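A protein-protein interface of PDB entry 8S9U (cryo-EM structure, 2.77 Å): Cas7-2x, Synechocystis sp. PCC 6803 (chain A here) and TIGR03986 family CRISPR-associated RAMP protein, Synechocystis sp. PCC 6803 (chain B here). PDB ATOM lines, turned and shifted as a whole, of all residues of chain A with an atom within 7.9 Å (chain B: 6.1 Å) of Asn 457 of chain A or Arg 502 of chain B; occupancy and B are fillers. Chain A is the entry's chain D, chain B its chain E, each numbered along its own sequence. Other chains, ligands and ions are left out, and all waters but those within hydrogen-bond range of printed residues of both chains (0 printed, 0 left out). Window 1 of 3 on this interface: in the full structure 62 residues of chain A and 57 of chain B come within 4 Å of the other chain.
O of His 504 of chain B is in hydrogen-bond range of N of Glu 634 of chain B. NH2 of Arg 458 of chain A sits close to OH of Tyr 454 of chain A (3.3 Å). The guanidinium group (NH1) of Arg 152 of chain B is in salt-bridge range of the side-chain carboxylate (OE1) of Glu 634 of chain B (2.8 Å). The guanidinium group of Arg 502 of chain B is in salt-bridge range of the side-chain carboxylate of Asp 636 of chain B, at 3.2 Å. The backbone NH (N) of Leu 501 of chain B sits at hydrogen-bond distance from the backbone carbonyl oxygen (O) of Val 485 of chain B (2.9 Å). A ring nitrogen (NE2) of His 141 of chain B sits at hydrogen-bond distance from the backbone carbonyl oxygen (O) of Lys 498 of chain B (2.7 Å).
The side-chain amino group (NZ) of Lys 448 of chain A lies within salt-bridge range of the side-chain carboxylate (OE2) of Glu 634 of chain B, 3.0 Å away. The backbone carbonyl oxygen of Gly 499 of chain B is in hydrogen-bond range of the side-chain amide nitrogen of Asn 457 of chain A (2.5 Å). The backbone carbonyl oxygen (O) of Asn 447 of chain A lies within hydrogen-bond range of the guanidinium group (NH2) of Arg 152 of chain B. O of Asn 457 of chain A lies within hydrogen-bond range of NZ of Lys 198 of chain B, 3.0 Å away. O of Lys 448 of chain A sits at hydrogen-bond distance from NH2 of Arg 502 of chain B, at 3.1 Å. NH2 of Arg 502 of chain B sits close to OG1 of Thr 462 of chain A (3.5 Å).
Printed residues of chain A that touch a printed residue of chain B: Asp 232, Asn 447, Lys 448, Pro 451, Thr 456, Asn 457, Arg 458 and Thr 462. Hydrophobic or aromatic side chains of chain B that line the printed part of chain A: His 504. Among the printed residues, 18 pairs touch across the chains. Among the printed residues, Asp or Glu carboxylates within 4 Å of a Lys or Arg side-chain nitrogen of the other chain: Lys 448 of chain A with Glu 634 of chain B.
Printed residues of chain B within 4 Å of Asn 447 of chain A: Arg 152 (2.7 Å). Printed residues of chain B within 4 Å of Thr 456 of chain A: Lys 498 (3.5 Å) and Arg 502 (3.5 Å). Asn 457 of chain A touches just these residues of chain B: Lys 198 (3.0 Å), Lys 498 (3.9 Å), Gly 499 (2.5 Å), Leu 501 (3.5 Å) and Arg 502 (3.4 Å). Of the printed residues of chain A, Thr 195 of chain B touches Arg 458 (3.2 Å). Of chain A, only Asn 457 (2.5 Å) comes within 4 Å of Gly 499 of chain B. Of the printed residues of chain A, Leu 501 of chain B touches Asn 457. Printed residues of chain A within 4 Å of His 504 of chain B: Asp 232, Lys 448 and Thr 462. Asp 636 of chain B touches none of the printed residues of chain A. Val 637 of chain B touches none of the printed residues of chain A. The nearest residue of chain B that does not touch Asn 457 of chain A is Gln 500 of chain B (4.3 Å).
Among the printed residues, pairs that only touch across the chains: Asp 232 of chain A with His 504 of chain B, Lys 448 of chain A with Arg 152 of chain B, Lys 448 of chain A with His 504 of chain B, Pro 451 of chain A with Arg 502 of chain B, Thr 456 of chain A with Lys 498 of chain B, Thr 456 of chain A with Arg 502 of chain B, Asn 457 of chain A with Lys 498 of chain B, Asn 457 of chain A with Leu 501 of chain B, Asn 457 of chain A with Arg 502 of chain B, Arg 458 of chain A with Thr 195 of chain B, Arg 458 of chain A with Lys 198 of chain B and Thr 462 of chain A with His 504 of chain B.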
ATOM      1  N   LYS A 231      30.543 -20.979  14.107  1.00  0.00           N
ATOM      2  CA  LYS A 231      29.717 -19.788  14.173  1.00  0.00           C
ATOM      3  C   LYS A 231      30.484 -18.735  14.954  1.00  0.00           C
ATOM      4  O   LYS A 231      30.658 -17.610  14.485  1.00  0.00           O
ATOM      5  CB  LYS A 231      28.369 -20.117  14.811  1.00  0.00           C
ATOM      6  CG  LYS A 231      27.456 -18.943  15.003  1.00  0.00           C
ATOM      7  CD  LYS A 231      27.028 -18.383  13.674  1.00  0.00           C
ATOM      8  CE  LYS A 231      25.870 -17.438  13.815  1.00  0.00           C
ATOM      9  NZ  LYS A 231      24.648 -18.168  14.203  1.00  0.00           N
ATOM     10  N   ASP A 232      30.883 -19.059  16.063  1.00  0.00           N
ATOM     11  CA  ASP A 232      31.888 -18.436  16.890  1.00  0.00           C
ATOM     12  C   ASP A 232      33.175 -19.223  16.725  1.00  0.00           C
ATOM     13  O   ASP A 232      33.121 -20.417  16.437  1.00  0.00           O
ATOM     14  CB  ASP A 232      31.483 -18.419  18.362  1.00  0.00           C
ATOM     15  CG  ASP A 232      30.291 -17.533  18.634  1.00  0.00           C
ATOM     16  OD1 ASP A 232      30.352 -16.323  18.343  1.00  0.00           O
ATOM     17  OD2 ASP A 232      29.290 -18.040  19.155  1.00  0.00           O
ATOM     18  N   ASN A 447      21.313 -27.869  17.071  1.00  0.00           N
ATOM     19  CA  ASN A 447      20.669 -26.691  17.633  1.00  0.00           C
ATOM     20  C   ASN A 447      21.606 -25.808  18.446  1.00  0.00           C
ATOM     21  O   ASN A 447      21.132 -25.040  19.282  1.00  0.00           O
ATOM     22  CB  ASN A 447      19.482 -27.115  18.485  1.00  0.00           C
ATOM     23  CG  ASN A 447      18.261 -27.370  17.660  1.00  0.00           C
ATOM     24  OD1 ASN A 447      17.570 -26.447  17.251  1.00  0.00           O
ATOM     25  ND2 ASN A 447      17.982 -28.631  17.409  1.00  0.00           N
ATOM     26  N   LYS A 448      22.912 -25.922  18.251  1.00  0.00           N
ATOM     27  CA  LYS A 448      23.945 -25.152  18.943  1.00  0.00           C
ATOM     28  C   LYS A 448      23.990 -25.395  20.442  1.00  0.00           C
ATOM     29  O   LYS A 448      24.618 -24.624  21.163  1.00  0.00           O
ATOM     30  CB  LYS A 448      23.849 -23.651  18.650  1.00  0.00           C
ATOM     31  CG  LYS A 448      23.659 -23.344  17.190  1.00  0.00           C
ATOM     32  CD  LYS A 448      23.803 -21.884  16.889  1.00  0.00           C
ATOM     33  CE  LYS A 448      22.714 -21.083  17.533  1.00  0.00           C
ATOM     34  NZ  LYS A 448      22.708 -19.696  17.017  1.00  0.00           N
ATOM     35  N   LYS A 449      23.319 -26.425  20.938  1.00  0.00           N
ATOM     36  CA  LYS A 449      23.358 -26.731  22.360  1.00  0.00           C
ATOM     37  C   LYS A 449      24.663 -27.358  22.819  1.00  0.00           C
ATOM     38  O   LYS A 449      24.881 -27.449  24.026  1.00  0.00           O
ATOM     39  CB  LYS A 449      22.213 -27.658  22.737  1.00  0.00           C
ATOM     40  CG  LYS A 449      20.892 -26.989  22.982  1.00  0.00           C
ATOM     41  CD  LYS A 449      19.836 -28.050  23.153  1.00  0.00           C
ATOM     42  CE  LYS A 449      18.557 -27.506  23.740  1.00  0.00           C
ATOM     43  NZ  LYS A 449      18.719 -27.309  25.213  1.00  0.00           N
ATOM     44  N   ILE A 450      25.518 -27.812  21.917  1.00  0.00           N
ATOM     45  CA  ILE A 450      26.805 -28.395  22.269  1.00  0.00           C
ATOM     46  C   ILE A 450      27.904 -27.566  21.626  1.00  0.00           C
ATOM     47  O   ILE A 450      28.155 -27.674  20.427  1.00  0.00           O
ATOM     48  CB  ILE A 450      26.903 -29.867  21.835  1.00  0.00           C
ATOM     49  CG1 ILE A 450      25.617 -30.612  22.152  1.00  0.00           C
ATOM     50  CG2 ILE A 450      28.048 -30.542  22.526  1.00  0.00           C
ATOM     51  CD1 ILE A 450      25.632 -32.016  21.698  1.00  0.00           C
ATOM     52  N   PRO A 451      28.557 -26.695  22.388  1.00  0.00           N
ATOM     53  CA  PRO A 451      29.765 -26.044  21.894  1.00  0.00           C
ATOM     54  C   PRO A 451      30.985 -26.933  22.040  1.00  0.00           C
ATOM     55  O   PRO A 451      31.061 -27.784  22.925  1.00  0.00           O
ATOM     56  CB  PRO A 451      29.870 -24.814  22.792  1.00  0.00           C
ATOM     57  CG  PRO A 451      29.294 -25.257  24.042  1.00  0.00           C
ATOM     58  CD  PRO A 451      28.193 -26.202  23.721  1.00  0.00           C
ATOM     59  N   VAL A 452      31.973 -26.695  21.188  1.00  0.00           N
ATOM     60  CA  VAL A 452      33.132 -27.569  21.105  1.00  0.00           C
ATOM     61  C   VAL A 452      34.401 -26.765  21.339  1.00  0.00           C
ATOM     62  O   VAL A 452      34.535 -25.634  20.868  1.00  0.00           O
ATOM     63  CB  VAL A 452      33.171 -28.318  19.755  1.00  0.00           C
ATOM     64  CG1 VAL A 452      33.079 -27.382  18.629  1.00  0.00           C
ATOM     65  CG2 VAL A 452      34.425 -29.148  19.628  1.00  0.00           C
ATOM     66  N   GLY A 453      35.329 -27.360  22.066  1.00  0.00           N
ATOM     67  CA  GLY A 453      36.652 -26.812  22.231  1.00  0.00           C
ATOM     68  C   GLY A 453      36.809 -25.851  23.391  1.00  0.00           C
ATOM     69  O   GLY A 453      36.048 -25.833  24.357  1.00  0.00           O
ATOM     70  N   TYR A 454      37.874 -25.065  23.293  1.00  0.00           N
ATOM     71  CA  TYR A 454      38.238 -24.101  24.316  1.00  0.00           C
ATOM     72  C   TYR A 454      37.259 -22.950  24.366  1.00  0.00           C
ATOM     73  O   TYR A 454      36.692 -22.548  23.352  1.00  0.00           O
ATOM     74  CB  TYR A 454      39.624 -23.543  24.034  1.00  0.00           C
ATOM     75  CG  TYR A 454      40.246 -22.809  25.180  1.00  0.00           C
ATOM     76  CD1 TYR A 454      40.569 -23.461  26.347  1.00  0.00           C
ATOM     77  CD2 TYR A 454      40.497 -21.454  25.097  1.00  0.00           C
ATOM     78  CE1 TYR A 454      41.128 -22.800  27.385  1.00  0.00           C
ATOM     79  CE2 TYR A 454      41.047 -20.784  26.132  1.00  0.00           C
ATOM     80  CZ  TYR A 454      41.367 -21.457  27.278  1.00  0.00           C
ATOM     81  OH  TYR A 454      41.938 -20.781  28.328  1.00  0.00           O
ATOM     82  N   GLY A 455      37.099 -22.390  25.558  1.00  0.00           N
ATOM     83  CA  GLY A 455      36.518 -21.076  25.691  1.00  0.00           C
ATOM     84  C   GLY A 455      35.066 -20.982  25.328  1.00  0.00           C
ATOM     85  O   GLY A 455      34.634 -19.944  24.843  1.00  0.00           O
ATOM     86  N   THR A 456      34.306 -22.059  25.503  1.00  0.00           N
ATOM     87  CA  THR A 456      32.938 -22.083  25.001  1.00  0.00           C
ATOM     88  C   THR A 456      32.072 -21.032  25.668  1.00  0.00           C
ATOM     89  O   THR A 456      31.183 -20.469  25.026  1.00  0.00           O
ATOM     90  CB  THR A 456      32.337 -23.468  25.170  1.00  0.00           C
ATOM     91  OG1 THR A 456      32.303 -23.809  26.553  1.00  0.00           O
ATOM     92  CG2 THR A 456      33.163 -24.458  24.451  1.00  0.00           C
ATOM     93  N   ASN A 457      32.318 -20.745  26.937  1.00  0.00           N
ATOM     94  CA  ASN A 457      31.583 -19.718  27.657  1.00  0.00           C
ATOM     95  C   ASN A 457      32.155 -18.333  27.448  1.00  0.00           C
ATOM     96  O   ASN A 457      31.581 -17.368  27.945  1.00  0.00           O
ATOM     97  CB  ASN A 457      31.579 -20.029  29.140  1.00  0.00           C
ATOM     98  CG  ASN A 457      30.337 -20.690  29.577  1.00  0.00           C
ATOM     99  OD1 ASN A 457      29.588 -21.204  28.774  1.00  0.00           O
ATOM    100  ND2 ASN A 457      30.097 -20.680  30.858  1.00  0.00           N
ATOM    101  N   ARG A 458      33.244 -18.209  26.703  1.00  0.00           N
ATOM    102  CA  ARG A 458      34.087 -17.024  26.659  1.00  0.00           C
ATOM    103  C   ARG A 458      34.371 -16.639  25.220  1.00  0.00           C
ATOM    104  O   ARG A 458      35.496 -16.332  24.833  1.00  0.00           O
ATOM    105  CB  ARG A 458      35.377 -17.211  27.454  1.00  0.00           C
ATOM    106  CG  ARG A 458      35.144 -17.649  28.879  1.00  0.00           C
ATOM    107  CD  ARG A 458      36.378 -17.590  29.739  1.00  0.00           C
ATOM    108  NE  ARG A 458      37.541 -18.293  29.218  1.00  0.00           N
ATOM    109  CZ  ARG A 458      37.650 -19.612  29.165  1.00  0.00           C
ATOM    110  NH1 ARG A 458      36.698 -20.370  29.654  1.00  0.00           N
ATOM    111  NH2 ARG A 458      38.737 -20.173  28.685  1.00  0.00           N
ATOM    112  N   GLY A 459      33.321 -16.640  24.410  1.00  0.00           N
ATOM    113  CA  GLY A 459      33.368 -16.120  23.065  1.00  0.00           C
ATOM    114  C   GLY A 459      33.726 -17.090  21.969  1.00  0.00           C
ATOM    115  O   GLY A 459      33.936 -16.658  20.831  1.00  0.00           O
ATOM    116  N   MET A 460      33.805 -18.380  22.260  1.00  0.00           N
ATOM    117  CA  MET A 460      34.261 -19.347  21.281  1.00  0.00           C
ATOM    118  C   MET A 460      33.372 -20.575  21.343  1.00  0.00           C
ATOM    119  O   MET A 460      32.549 -20.723  22.239  1.00  0.00           O
ATOM    120  CB  MET A 460      35.729 -19.701  21.504  1.00  0.00           C
ATOM    121  CG  MET A 460      36.665 -18.561  21.165  1.00  0.00           C
ATOM    122  SD  MET A 460      38.310 -19.074  20.688  1.00  0.00           S
ATOM    123  CE  MET A 460      38.814 -19.914  22.168  1.00  0.00           C
ATOM    124  N   GLY A 461      33.526 -21.448  20.363  1.00  0.00           N
ATOM    125  CA  GLY A 461      33.027 -22.802  20.441  1.00  0.00           C
ATOM    126  C   GLY A 461      31.654 -23.080  19.875  1.00  0.00           C
ATOM    127  O   GLY A 461      31.228 -24.231  19.896  1.00  0.00           O
ATOM    128  N   THR A 462      30.963 -22.101  19.320  1.00  0.00           N
ATOM    129  CA  THR A 462      29.641 -22.341  18.766  1.00  0.00           C
ATOM    130  C   THR A 462      29.747 -22.751  17.313  1.00  0.00           C
ATOM    131  O   THR A 462      30.435 -22.101  16.525  1.00  0.00           O
ATOM    132  CB  THR A 462      28.755 -21.108  18.881  1.00  0.00           C
ATOM    133  OG1 THR A 462      28.983 -20.469  20.138  1.00  0.00           O
ATOM    134  CG2 THR A 462      27.316 -21.468  18.734  1.00  0.00           C
ATOM    135  N   ILE A 463      29.061 -23.822  16.961  1.00  0.00           N
ATOM    136  CA  ILE A 463      29.148 -24.385  15.627  1.00  0.00           C
ATOM    137  C   ILE A 463      27.775 -24.306  14.998  1.00  0.00           C
ATOM    138  O   ILE A 463      26.755 -24.296  15.687  1.00  0.00           O
ATOM    139  CB  ILE A 463      29.661 -25.835  15.627  1.00  0.00           C
ATOM    140  CG1 ILE A 463      28.660 -26.768  16.270  1.00  0.00           C
ATOM    141  CG2 ILE A 463      30.900 -25.924  16.420  1.00  0.00           C
ATOM    142  CD1 ILE A 463      29.057 -28.197  16.166  1.00  0.00           C
ATOM    143  N   HIS B 141      26.135 -28.644  36.332  1.00  0.00           N
ATOM    144  CA  HIS B 141      25.928 -28.850  34.911  1.00  0.00           C
ATOM    145  C   HIS B 141      25.456 -30.252  34.558  1.00  0.00           C
ATOM    146  O   HIS B 141      25.327 -30.552  33.374  1.00  0.00           O
ATOM    147  CB  HIS B 141      27.230 -28.558  34.160  1.00  0.00           C
ATOM    148  CG  HIS B 141      27.636 -27.119  34.187  1.00  0.00           C
ATOM    149  ND1 HIS B 141      27.125 -26.183  33.321  1.00  0.00           N
ATOM    150  CD2 HIS B 141      28.506 -26.459  34.978  1.00  0.00           C
ATOM    151  CE1 HIS B 141      27.655 -25.007  33.587  1.00  0.00           C
ATOM    152  NE2 HIS B 141      28.495 -25.147  34.589  1.00  0.00           N
ATOM    153  N   ARG B 152      17.603 -20.787  25.788  1.00  0.00           N
ATOM    154  CA  ARG B 152      18.173 -19.751  24.943  1.00  0.00           C
ATOM    155  C   ARG B 152      17.411 -18.457  25.164  1.00  0.00           C
ATOM    156  O   ARG B 152      16.182 -18.456  25.151  1.00  0.00           O
ATOM    157  CB  ARG B 152      18.062 -20.153  23.472  1.00  0.00           C
ATOM    158  CG  ARG B 152      18.872 -19.346  22.493  1.00  0.00           C
ATOM    159  CD  ARG B 152      20.330 -19.688  22.520  1.00  0.00           C
ATOM    160  NE  ARG B 152      20.583 -21.105  22.269  1.00  0.00           N
ATOM    161  CZ  ARG B 152      20.354 -21.721  21.114  1.00  0.00           C
ATOM    162  NH1 ARG B 152      19.940 -21.043  20.057  1.00  0.00           N
ATOM    163  NH2 ARG B 152      20.615 -23.009  20.995  1.00  0.00           N
ATOM    164  N   THR B 195      33.001 -11.848  24.658  1.00  0.00           N
ATOM    165  CA  THR B 195      33.682 -11.527  25.909  1.00  0.00           C
ATOM    166  C   THR B 195      33.446 -10.088  26.339  1.00  0.00           C
ATOM    167  O   THR B 195      33.349  -9.804  27.533  1.00  0.00           O
ATOM    168  CB  THR B 195      35.168 -11.816  25.784  1.00  0.00           C
ATOM    169  OG1 THR B 195      35.664 -11.248  24.573  1.00  0.00           O
ATOM    170  CG2 THR B 195      35.399 -13.280  25.757  1.00  0.00           C
ATOM    171  N   LYS B 198      29.934 -10.106  27.532  1.00  0.00           N
ATOM    172  CA  LYS B 198      29.876 -10.827  28.796  1.00  0.00           C
ATOM    173  C   LYS B 198      30.420 -10.010  29.952  1.00  0.00           C
ATOM    174  O   LYS B 198      29.884 -10.071  31.060  1.00  0.00           O
ATOM    175  CB  LYS B 198      30.656 -12.129  28.688  1.00  0.00           C
ATOM    176  CG  LYS B 198      30.483 -13.051  29.854  1.00  0.00           C
ATOM    177  CD  LYS B 198      31.295 -14.289  29.679  1.00  0.00           C
ATOM    178  CE  LYS B 198      31.048 -15.232  30.809  1.00  0.00           C
ATOM    179  NZ  LYS B 198      31.963 -16.380  30.787  1.00  0.00           N
ATOM    180  N   VAL B 485      26.380 -17.789  38.005  1.00  0.00           N
ATOM    181  CA  VAL B 485      25.847 -17.514  36.680  1.00  0.00           C
ATOM    182  C   VAL B 485      26.961 -17.408  35.649  1.00  0.00           C
ATOM    183  O   VAL B 485      26.908 -18.041  34.595  1.00  0.00           O
ATOM    184  CB  VAL B 485      24.994 -16.240  36.715  1.00  0.00           C
ATOM    185  CG1 VAL B 485      24.522 -15.901  35.351  1.00  0.00           C
ATOM    186  CG2 VAL B 485      23.826 -16.452  37.612  1.00  0.00           C
ATOM    187  N   PHE B 486      27.985 -16.609  35.923  1.00  0.00           N
ATOM    188  CA  PHE B 486      29.065 -16.434  34.968  1.00  0.00           C
ATOM    189  C   PHE B 486      30.273 -17.315  35.220  1.00  0.00           C
ATOM    190  O   PHE B 486      31.132 -17.408  34.349  1.00  0.00           O
ATOM    191  CB  PHE B 486      29.491 -14.976  34.917  1.00  0.00           C
ATOM    192  CG  PHE B 486      28.432 -14.070  34.410  1.00  0.00           C
ATOM    193  CD1 PHE B 486      27.449 -13.605  35.243  1.00  0.00           C
ATOM    194  CD2 PHE B 486      28.410 -13.690  33.096  1.00  0.00           C
ATOM    195  CE1 PHE B 486      26.479 -12.785  34.779  1.00  0.00           C
ATOM    196  CE2 PHE B 486      27.438 -12.866  32.635  1.00  0.00           C
ATOM    197  CZ  PHE B 486      26.470 -12.417  33.478  1.00  0.00           C
ATOM    198  N   LYS B 498      32.502 -23.813  35.882  1.00  0.00           N
ATOM    199  CA  LYS B 498      32.083 -23.353  34.568  1.00  0.00           C
ATOM    200  C   LYS B 498      30.816 -22.525  34.672  1.00  0.00           C
ATOM    201  O   LYS B 498      29.847 -22.931  35.305  1.00  0.00           O
ATOM    202  CB  LYS B 498      31.865 -24.521  33.626  1.00  0.00           C
ATOM    203  CG  LYS B 498      31.609 -24.054  32.235  1.00  0.00           C
ATOM    204  CD  LYS B 498      31.351 -25.164  31.297  1.00  0.00           C
ATOM    205  CE  LYS B 498      31.162 -24.597  29.934  1.00  0.00           C
ATOM    206  NZ  LYS B 498      30.523 -25.554  29.015  1.00  0.00           N
ATOM    207  N   GLY B 499      30.829 -21.354  34.051  1.00  0.00           N
ATOM    208  CA  GLY B 499      29.678 -20.478  34.122  1.00  0.00           C
ATOM    209  C   GLY B 499      28.443 -21.087  33.494  1.00  0.00           C
ATOM    210  O   GLY B 499      28.507 -21.761  32.468  1.00  0.00           O
ATOM    211  N   GLN B 500      27.314 -20.860  34.133  1.00  0.00           N
ATOM    212  CA  GLN B 500      25.995 -21.235  33.658  1.00  0.00           C
ATOM    213  C   GLN B 500      25.439 -20.309  32.590  1.00  0.00           C
ATOM    214  O   GLN B 500      24.271 -20.435  32.244  1.00  0.00           O
ATOM    215  CB  GLN B 500      25.047 -21.306  34.842  1.00  0.00           C
ATOM    216  CG  GLN B 500      25.209 -22.562  35.625  1.00  0.00           C
ATOM    217  CD  GLN B 500      24.514 -22.491  36.935  1.00  0.00           C
ATOM    218  OE1 GLN B 500      25.118 -22.696  37.975  1.00  0.00           O
ATOM    219  NE2 GLN B 500      23.255 -22.131  36.910  1.00  0.00           N
ATOM    220  N   LEU B 501      26.212 -19.363  32.076  1.00  0.00           N
ATOM    221  CA  LEU B 501      25.717 -18.406  31.096  1.00  0.00           C
ATOM    222  C   LEU B 501      26.717 -18.312  29.958  1.00  0.00           C
ATOM    223  O   LEU B 501      27.895 -18.028  30.187  1.00  0.00           O
ATOM    224  CB  LEU B 501      25.478 -17.042  31.750  1.00  0.00           C
ATOM    225  CG  LEU B 501      24.845 -15.900  30.973  1.00  0.00           C
ATOM    226  CD1 LEU B 501      24.302 -14.909  31.935  1.00  0.00           C
ATOM    227  CD2 LEU B 501      25.862 -15.206  30.120  1.00  0.00           C
ATOM    228  N   ARG B 502      26.244 -18.545  28.739  1.00  0.00           N
ATOM    229  CA  ARG B 502      27.061 -18.549  27.533  1.00  0.00           C
ATOM    230  C   ARG B 502      26.512 -17.533  26.548  1.00  0.00           C
ATOM    231  O   ARG B 502      25.368 -17.651  26.115  1.00  0.00           O
ATOM    232  CB  ARG B 502      27.067 -19.940  26.913  1.00  0.00           C
ATOM    233  CG  ARG B 502      27.661 -20.016  25.567  1.00  0.00           C
ATOM    234  CD  ARG B 502      27.798 -21.438  25.146  1.00  0.00           C
ATOM    235  NE  ARG B 502      27.663 -21.590  23.705  1.00  0.00           N
ATOM    236  CZ  ARG B 502      26.784 -22.407  23.134  1.00  0.00           C
ATOM    237  NH1 ARG B 502      25.913 -23.074  23.875  1.00  0.00           N
ATOM    238  NH2 ARG B 502      26.722 -22.504  21.820  1.00  0.00           N
ATOM    239  N   ILE B 503      27.323 -16.551  26.181  1.00  0.00           N
ATOM    240  CA  ILE B 503      26.975 -15.591  25.141  1.00  0.00           C
ATOM    241  C   ILE B 503      27.584 -16.054  23.833  1.00  0.00           C
ATOM    242  O   ILE B 503      28.760 -16.426  23.787  1.00  0.00           O
ATOM    243  CB  ILE B 503      27.451 -14.178  25.505  1.00  0.00           C
ATOM    244  CG1 ILE B 503      26.840 -13.771  26.836  1.00  0.00           C
ATOM    245  CG2 ILE B 503      27.088 -13.208  24.429  1.00  0.00           C
ATOM    246  CD1 ILE B 503      26.985 -12.355  27.154  1.00  0.00           C
ATOM    247  N   HIS B 504      26.790 -16.047  22.772  1.00  0.00           N
ATOM    248  CA  HIS B 504      27.229 -16.623  21.515  1.00  0.00           C
ATOM    249  C   HIS B 504      26.417 -16.023  20.382  1.00  0.00           C
ATOM    250  O   HIS B 504      25.475 -15.267  20.601  1.00  0.00           O
ATOM    251  CB  HIS B 504      27.133 -18.146  21.546  1.00  0.00           C
ATOM    252  CG  HIS B 504      25.736 -18.672  21.574  1.00  0.00           C
ATOM    253  ND1 HIS B 504      25.022 -18.942  20.431  1.00  0.00           N
ATOM    254  CD2 HIS B 504      24.924 -18.984  22.606  1.00  0.00           C
ATOM    255  CE1 HIS B 504      23.829 -19.395  20.757  1.00  0.00           C
ATOM    256  NE2 HIS B 504      23.743 -19.428  22.071  1.00  0.00           N
ATOM    257  N   GLU B 634      22.845 -14.210  21.270  1.00  0.00           N
ATOM    258  CA  GLU B 634      22.041 -15.120  22.058  1.00  0.00           C
ATOM    259  C   GLU B 634      22.737 -15.444  23.364  1.00  0.00           C
ATOM    260  O   GLU B 634      23.960 -15.518  23.428  1.00  0.00           O
ATOM    261  CB  GLU B 634      21.770 -16.389  21.271  1.00  0.00           C
ATOM    262  CG  GLU B 634      20.897 -16.121  20.076  1.00  0.00           C
ATOM    263  CD  GLU B 634      20.788 -17.296  19.155  1.00  0.00           C
ATOM    264  OE1 GLU B 634      20.092 -18.265  19.511  1.00  0.00           O
ATOM    265  OE2 GLU B 634      21.403 -17.260  18.074  1.00  0.00           O
ATOM    266  N   ILE B 635      21.945 -15.641  24.408  1.00  0.00           N
ATOM    267  CA  ILE B 635      22.431 -16.127  25.688  1.00  0.00           C
ATOM    268  C   ILE B 635      21.839 -17.508  25.897  1.00  0.00           C
ATOM    269  O   ILE B 635      20.618 -17.675  25.880  1.00  0.00           O
ATOM    270  CB  ILE B 635      22.042 -15.185  26.833  1.00  0.00           C
ATOM    271  CG1 ILE B 635      22.363 -13.748  26.468  1.00  0.00           C
ATOM    272  CG2 ILE B 635      22.769 -15.549  28.081  1.00  0.00           C
ATOM    273  CD1 ILE B 635      22.013 -12.788  27.527  1.00  0.00           C
ATOM    274  N   ASP B 636      22.698 -18.488  26.105  1.00  0.00           N
ATOM    275  CA  ASP B 636      22.294 -19.831  26.479  1.00  0.00           C
ATOM    276  C   ASP B 636      22.560 -19.990  27.969  1.00  0.00           C
ATOM    277  O   ASP B 636      23.699 -19.848  28.410  1.00  0.00           O
ATOM    278  CB  ASP B 636      23.062 -20.845  25.633  1.00  0.00           C
ATOM    279  CG  ASP B 636      22.952 -22.262  26.143  1.00  0.00           C
ATOM    280  OD1 ASP B 636      21.825 -22.801  26.198  1.00  0.00           O
ATOM    281  OD2 ASP B 636      24.003 -22.854  26.471  1.00  0.00           O
ATOM    282  N   VAL B 637      21.522 -20.300  28.735  1.00  0.00           N
ATOM    283  CA  VAL B 637      21.606 -20.332  30.189  1.00  0.00           C
ATOM    284  C   VAL B 637      21.289 -21.727  30.691  1.00  0.00           C
ATOM    285  O   VAL B 637      20.552 -22.484  30.059  1.00  0.00           O
ATOM    286  CB  VAL B 637      20.667 -19.303  30.851  1.00  0.00           C
ATOM    287  CG1 VAL B 637      20.970 -17.913  30.352  1.00  0.00           C
ATOM    288  CG2 VAL B 637      19.233 -19.651  30.602  1.00  0.00           C
